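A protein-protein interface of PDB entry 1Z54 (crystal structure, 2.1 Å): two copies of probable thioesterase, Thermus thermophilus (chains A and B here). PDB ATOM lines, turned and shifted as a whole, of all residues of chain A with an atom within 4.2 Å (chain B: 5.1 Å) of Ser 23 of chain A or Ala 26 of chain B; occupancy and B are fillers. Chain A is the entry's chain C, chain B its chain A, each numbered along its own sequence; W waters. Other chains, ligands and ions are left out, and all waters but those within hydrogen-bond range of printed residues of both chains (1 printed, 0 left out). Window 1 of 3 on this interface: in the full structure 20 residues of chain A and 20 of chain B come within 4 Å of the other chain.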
ATOM      1  N   HIS A  21     -13.170 -14.638 -38.535  1.00  0.00           N
ATOM      2  CA  HIS A  21     -12.754 -15.656 -37.576  1.00  0.00           C
ATOM      3  C   HIS A  21     -13.968 -16.304 -36.912  1.00  0.00           C
ATOM      4  O   HIS A  21     -14.911 -15.615 -36.515  1.00  0.00           O
ATOM      5  CB  HIS A  21     -11.822 -15.041 -36.532  1.00  0.00           C
ATOM      6  CG  HIS A  21     -11.087 -16.055 -35.719  1.00  0.00           C
ATOM      7  ND1 HIS A  21     -11.535 -16.491 -34.489  1.00  0.00           N
ATOM      8  CD2 HIS A  21      -9.944 -16.737 -35.969  1.00  0.00           C
ATOM      9  CE1 HIS A  21     -10.695 -17.393 -34.014  1.00  0.00           C
ATOM     10  NE2 HIS A  21      -9.722 -17.561 -34.892  1.00  0.00           N
ATOM     11  N   HIS A  22     -13.942 -17.629 -36.786  1.00  0.00           N
ATOM     12  CA  HIS A  22     -15.071 -18.348 -36.205  1.00  0.00           C
ATOM     13  C   HIS A  22     -15.489 -17.853 -34.828  1.00  0.00           C
ATOM     14  O   HIS A  22     -16.642 -18.012 -34.436  1.00  0.00           O
ATOM     15  CB  HIS A  22     -14.780 -19.852 -36.159  1.00  0.00           C
ATOM     16  CG  HIS A  22     -13.573 -20.212 -35.344  1.00  0.00           C
ATOM     17  ND1 HIS A  22     -13.654 -20.573 -34.018  1.00  0.00           N
ATOM     18  CD2 HIS A  22     -12.258 -20.246 -35.664  1.00  0.00           C
ATOM     19  CE1 HIS A  22     -12.441 -20.814 -33.553  1.00  0.00           C
ATOM     20  NE2 HIS A  22     -11.574 -20.623 -34.533  1.00  0.00           N
ATOM     21  N   SER A  23     -14.570 -17.238 -34.090  1.00  0.00           N
ATOM     22  CA  SER A  23     -14.917 -16.742 -32.763  1.00  0.00           C
ATOM     23  C   SER A  23     -15.791 -15.481 -32.799  1.00  0.00           C
ATOM     24  O   SER A  23     -16.497 -15.182 -31.827  1.00  0.00           O
ATOM     25  CB  SER A  23     -13.653 -16.468 -31.953  1.00  0.00           C
ATOM     26  OG  SER A  23     -13.009 -15.278 -32.376  1.00  0.00           O
ATOM     27  N   VAL A  24     -15.753 -14.758 -33.918  1.00  0.00           N
ATOM     28  CA  VAL A  24     -16.530 -13.526 -34.073  1.00  0.00           C
ATOM     29  C   VAL A  24     -18.035 -13.794 -34.152  1.00  0.00           C
ATOM     30  O   VAL A  24     -18.851 -12.993 -33.685  1.00  0.00           O
ATOM     31  CB  VAL A  24     -16.110 -12.755 -35.364  1.00  0.00           C
ATOM     32  CG1 VAL A  24     -16.952 -11.488 -35.526  1.00  0.00           C
ATOM     33  CG2 VAL A  24     -14.629 -12.398 -35.308  1.00  0.00           C
ATOM     34  N   TYR A  25     -18.393 -14.929 -34.739  1.00  0.00           N
ATOM     35  CA  TYR A  25     -19.790 -15.294 -34.917  1.00  0.00           C
ATOM     36  C   TYR A  25     -20.630 -15.218 -33.654  1.00  0.00           C
ATOM     37  O   TYR A  25     -21.799 -14.829 -33.706  1.00  0.00           O
ATOM     38  CB  TYR A  25     -19.869 -16.681 -35.541  1.00  0.00           C
ATOM     39  CG  TYR A  25     -19.554 -16.651 -37.010  1.00  0.00           C
ATOM     40  CD1 TYR A  25     -20.577 -16.572 -37.961  1.00  0.00           C
ATOM     41  CD2 TYR A  25     -18.233 -16.658 -37.460  1.00  0.00           C
ATOM     42  CE1 TYR A  25     -20.288 -16.500 -39.327  1.00  0.00           C
ATOM     43  CE2 TYR A  25     -17.936 -16.590 -38.816  1.00  0.00           C
ATOM     44  CZ  TYR A  25     -18.968 -16.511 -39.744  1.00  0.00           C
ATOM     45  OH  TYR A  25     -18.675 -16.441 -41.091  1.00  0.00           O
ATOM     46  N   ALA A  26     -20.033 -15.577 -32.524  1.00  0.00           N
ATOM     47  CA  ALA A  26     -20.739 -15.525 -31.258  1.00  0.00           C
ATOM     48  C   ALA A  26     -21.103 -14.070 -30.974  1.00  0.00           C
ATOM     49  O   ALA A  26     -22.160 -13.780 -30.416  1.00  0.00           O
ATOM     50  CB  ALA A  26     -19.852 -16.092 -30.135  1.00  0.00           C
ATOM     51  N   HIS B  22     -18.383 -14.862 -22.941  1.00  0.00           N
ATOM     52  CA  HIS B  22     -18.530 -16.172 -23.552  1.00  0.00           C
ATOM     53  C   HIS B  22     -17.915 -16.338 -24.943  1.00  0.00           C
ATOM     54  O   HIS B  22     -17.562 -17.459 -25.328  1.00  0.00           O
ATOM     55  CB  HIS B  22     -20.006 -16.585 -23.561  1.00  0.00           C
ATOM     56  CG  HIS B  22     -20.883 -15.698 -24.385  1.00  0.00           C
ATOM     57  ND1 HIS B  22     -21.207 -15.983 -25.694  1.00  0.00           N
ATOM     58  CD2 HIS B  22     -21.512 -14.537 -24.085  1.00  0.00           C
ATOM     59  CE1 HIS B  22     -22.002 -15.038 -26.163  1.00  0.00           C
ATOM     60  NE2 HIS B  22     -22.203 -14.150 -25.206  1.00  0.00           N
ATOM     61  N   SER B  23     -17.775 -15.251 -25.703  1.00  0.00           N
ATOM     62  CA  SER B  23     -17.184 -15.380 -27.040  1.00  0.00           C
ATOM     63  C   SER B  23     -15.677 -15.587 -26.946  1.00  0.00           C
ATOM     64  O   SER B  23     -15.057 -16.130 -27.857  1.00  0.00           O
ATOM     65  CB  SER B  23     -17.473 -14.150 -27.915  1.00  0.00           C
ATOM     66  OG  SER B  23     -16.743 -13.006 -27.502  1.00  0.00           O
ATOM     67  N   VAL B  24     -15.092 -15.166 -25.832  1.00  0.00           N
ATOM     68  CA  VAL B  24     -13.656 -15.302 -25.628  1.00  0.00           C
ATOM     69  C   VAL B  24     -13.209 -16.761 -25.521  1.00  0.00           C
ATOM     70  O   VAL B  24     -12.114 -17.118 -25.953  1.00  0.00           O
ATOM     71  CB  VAL B  24     -13.226 -14.516 -24.369  1.00  0.00           C
ATOM     72  CG1 VAL B  24     -11.770 -14.794 -24.024  1.00  0.00           C
ATOM     73  CG2 VAL B  24     -13.413 -13.031 -24.621  1.00  0.00           C
ATOM     74  N   TYR B  25     -14.068 -17.616 -24.976  1.00  0.00           N
ATOM     75  CA  TYR B  25     -13.708 -19.021 -24.810  1.00  0.00           C
ATOM     76  C   TYR B  25     -13.251 -19.733 -26.083  1.00  0.00           C
ATOM     77  O   TYR B  25     -12.332 -20.554 -26.042  1.00  0.00           O
ATOM     78  CB  TYR B  25     -14.864 -19.765 -24.146  1.00  0.00           C
ATOM     79  CG  TYR B  25     -15.012 -19.421 -22.672  1.00  0.00           C
ATOM     80  CD1 TYR B  25     -14.510 -20.268 -21.682  1.00  0.00           C
ATOM     81  CD2 TYR B  25     -15.651 -18.243 -22.269  1.00  0.00           C
ATOM     82  CE1 TYR B  25     -14.641 -19.955 -20.322  1.00  0.00           C
ATOM     83  CE2 TYR B  25     -15.789 -17.919 -20.915  1.00  0.00           C
ATOM     84  CZ  TYR B  25     -15.286 -18.781 -19.948  1.00  0.00           C
ATOM     85  OH  TYR B  25     -15.446 -18.474 -18.611  1.00  0.00           O
ATOM     86  N   ALA B  26     -13.860 -19.416 -27.219  1.00  0.00           N
ATOM     87  CA  ALA B  26     -13.448 -20.052 -28.466  1.00  0.00           C
ATOM     88  C   ALA B  26     -11.988 -19.691 -28.758  1.00  0.00           C
ATOM     89  O   ALA B  26     -11.258 -20.480 -29.345  1.00  0.00           O
ATOM     90  CB  ALA B  26     -14.343 -19.603 -29.621  1.00  0.00           C
ATOM     91  N   VAL B  27     -11.572 -18.492 -28.357  1.00  0.00           N
ATOM     92  CA  VAL B  27     -10.198 -18.062 -28.574  1.00  0.00           C
ATOM     93  C   VAL B  27      -9.274 -18.882 -27.662  1.00  0.00           C
ATOM     94  O   VAL B  27      -8.188 -19.298 -28.078  1.00  0.00           O
ATOM     95  CB  VAL B  27     -10.035 -16.548 -28.294  1.00  0.00           C
ATOM     96  CG1 VAL B  27      -8.567 -16.161 -28.305  1.00  0.00           C
ATOM     97  CG2 VAL B  27     -10.780 -15.744 -29.370  1.00  0.00           C
ATOM     98  N   TYR B  28      -9.713 -19.114 -26.426  1.00  0.00           N
ATOM     99  CA  TYR B  28      -8.940 -19.918 -25.476  1.00  0.00           C
ATOM    100  C   TYR B  28      -8.814 -21.332 -26.038  1.00  0.00           C
ATOM    101  O   TYR B  28      -7.756 -21.949 -25.948  1.00  0.00           O
ATOM    102  CB  TYR B  28      -9.646 -19.990 -24.123  1.00  0.00           C
ATOM    103  CG  TYR B  28      -9.648 -18.721 -23.303  1.00  0.00           C
ATOM    104  CD1 TYR B  28     -10.352 -18.666 -22.096  1.00  0.00           C
ATOM    105  CD2 TYR B  28      -8.942 -17.585 -23.702  1.00  0.00           C
ATOM    106  CE1 TYR B  28     -10.357 -17.525 -21.312  1.00  0.00           C
ATOM    107  CE2 TYR B  28      -8.940 -16.428 -22.914  1.00  0.00           C
ATOM    108  CZ  TYR B  28      -9.652 -16.412 -21.714  1.00  0.00           C
ATOM    109  OH  TYR B  28      -9.647 -15.306 -20.878  1.00  0.00           O
ATOM    110  N   LEU B  29      -9.896 -21.847 -26.620  1.00  0.00           N
ATOM    111  CA  LEU B  29      -9.869 -23.183 -27.216  1.00  0.00           C
ATOM    112  C   LEU B  29      -8.867 -23.229 -28.370  1.00  0.00           C
ATOM    113  O   LEU B  29      -8.145 -24.211 -28.542  1.00  0.00           O
ATOM    114  CB  LEU B  29     -11.257 -23.581 -27.745  1.00  0.00           C
ATOM    115  CG  LEU B  29     -12.389 -23.722 -26.715  1.00  0.00           C
ATOM    116  CD1 LEU B  29     -13.575 -24.434 -27.343  1.00  0.00           C
ATOM    117  CD2 LEU B  29     -11.896 -24.514 -25.507  1.00  0.00           C
ATOM    118  N   GLU B  30      -8.847 -22.168 -29.170  1.00  0.00           N
ATOM    119  CA  GLU B  30      -7.940 -22.088 -30.306  1.00  0.00           C
ATOM    120  C   GLU B  30      -6.490 -22.068 -29.825  1.00  0.00           C
ATOM    121  O   GLU B  30      -5.639 -22.754 -30.377  1.00  0.00           O
ATOM    122  CB  GLU B  30      -8.242 -20.834 -31.138  1.00  0.00           C
ATOM    123  CG  GLU B  30      -7.278 -20.596 -32.314  1.00  0.00           C
ATOM    124  CD  GLU B  30      -7.634 -19.343 -33.121  1.00  0.00           C
ATOM    125  OE1 GLU B  30      -8.172 -19.472 -34.244  1.00  0.00           O
ATOM    126  OE2 GLU B  30      -7.387 -18.226 -32.616  1.00  0.00           O
ATOM    127  N   LEU B  59     -18.605 -25.543 -33.611  1.00  0.00           N
ATOM    128  CA  LEU B  59     -18.123 -25.202 -32.279  1.00  0.00           C
ATOM    129  C   LEU B  59     -19.230 -25.492 -31.275  1.00  0.00           C
ATOM    130  O   LEU B  59     -20.417 -25.356 -31.581  1.00  0.00           O
ATOM    131  CB  LEU B  59     -17.746 -23.716 -32.215  1.00  0.00           C
ATOM    132  CG  LEU B  59     -17.519 -23.095 -30.832  1.00  0.00           C
ATOM    133  CD1 LEU B  59     -16.252 -23.666 -30.204  1.00  0.00           C
ATOM    134  CD2 LEU B  59     -17.401 -21.575 -30.967  1.00  0.00           C
ATOM    135  N   LEU B  61     -19.880 -25.113 -26.873  1.00  0.00           N
ATOM    136  CA  LEU B  61     -19.371 -24.763 -25.560  1.00  0.00           C
ATOM    137  C   LEU B  61     -20.448 -24.756 -24.496  1.00  0.00           C
ATOM    138  O   LEU B  61     -21.544 -24.231 -24.704  1.00  0.00           O
ATOM    139  CB  LEU B  61     -18.691 -23.388 -25.594  1.00  0.00           C
ATOM    140  CG  LEU B  61     -17.186 -23.359 -25.881  1.00  0.00           C
ATOM    141  CD1 LEU B  61     -16.800 -22.009 -26.449  1.00  0.00           C
ATOM    142  CD2 LEU B  61     -16.404 -23.655 -24.598  1.00  0.00           C
HETATM  143  O   HOH W   1     -16.606 -16.991 -29.786  1.00  0.00           O
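OE1 of Glu 30 of chain B is in hydrogen-bond range of NE2 of His 21 of chain A, 2.5 Å away.
A ring nitrogen (ND1) of His 21 of chain A is in hydrogen-bond range of the side-chain hydroxyl (OG) of Ser 23 of chain A (2.8 Å).
OE1 of Glu 30 of chain B touches NE2 of His 22 of chain A, at 3.6 Å. CB of Ala 26 of chain B touches CB of Ser 23 of chain A, 3.97 Å away. CG2 of Val 27 of chain B touches OG of Ser 23 of chain A (3.8 Å). CB of Ala 26 of chain A touches CB of Ser 23 of chain B (3.8 Å).
Of the printed residues of chain B, His 21 of chain A touches Glu 30 (2.5 Å). Of the printed residues of chain B, His 22 of chain A touches Glu 30 (3.6 Å). Ser 23 of chain A touches two residues of chain B. Ala 26 of chain B touches just one residue of chain A: Ser 23 (3.97 Å). Of the printed residues of chain A, Val 27 of chain B touches Ser 23. Tyr 28 of chain B touches none of the printed residues of chain A. The nearest residue of chain B that does not touch Ser 23 of chain A is Ser 23 of chain B (4.2 Å). The nearest printed residue of chain A that does not touch Ser 23 of chain B is Ser 23 of chain A (4.2 Å).
Of the 6 printed residues of chain A, 4 touch a printed residue of chain B. Among the printed residues, no Asp or Glu carboxylate lies within 4 Å of a Lys or Arg side-chain nitrogen of the other chain.
Ser 23 of chain A touches Ala 26 of chain B, and with the chains exchanged Ala 26 of chain A touches Ser 23 of chain B. 5 positions are printed for both chains. Of the 5 pairs that touch across the chains among the printed residues, 2 have their exchanged pair printed and touching as well.
Water W1 bridges the backbone carbonyl oxygen (O) of Ser 23 of chain B (2.6 Å) and the backbone carbonyl oxygen (O) of Ser 23 of chain A (2.7 Å).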
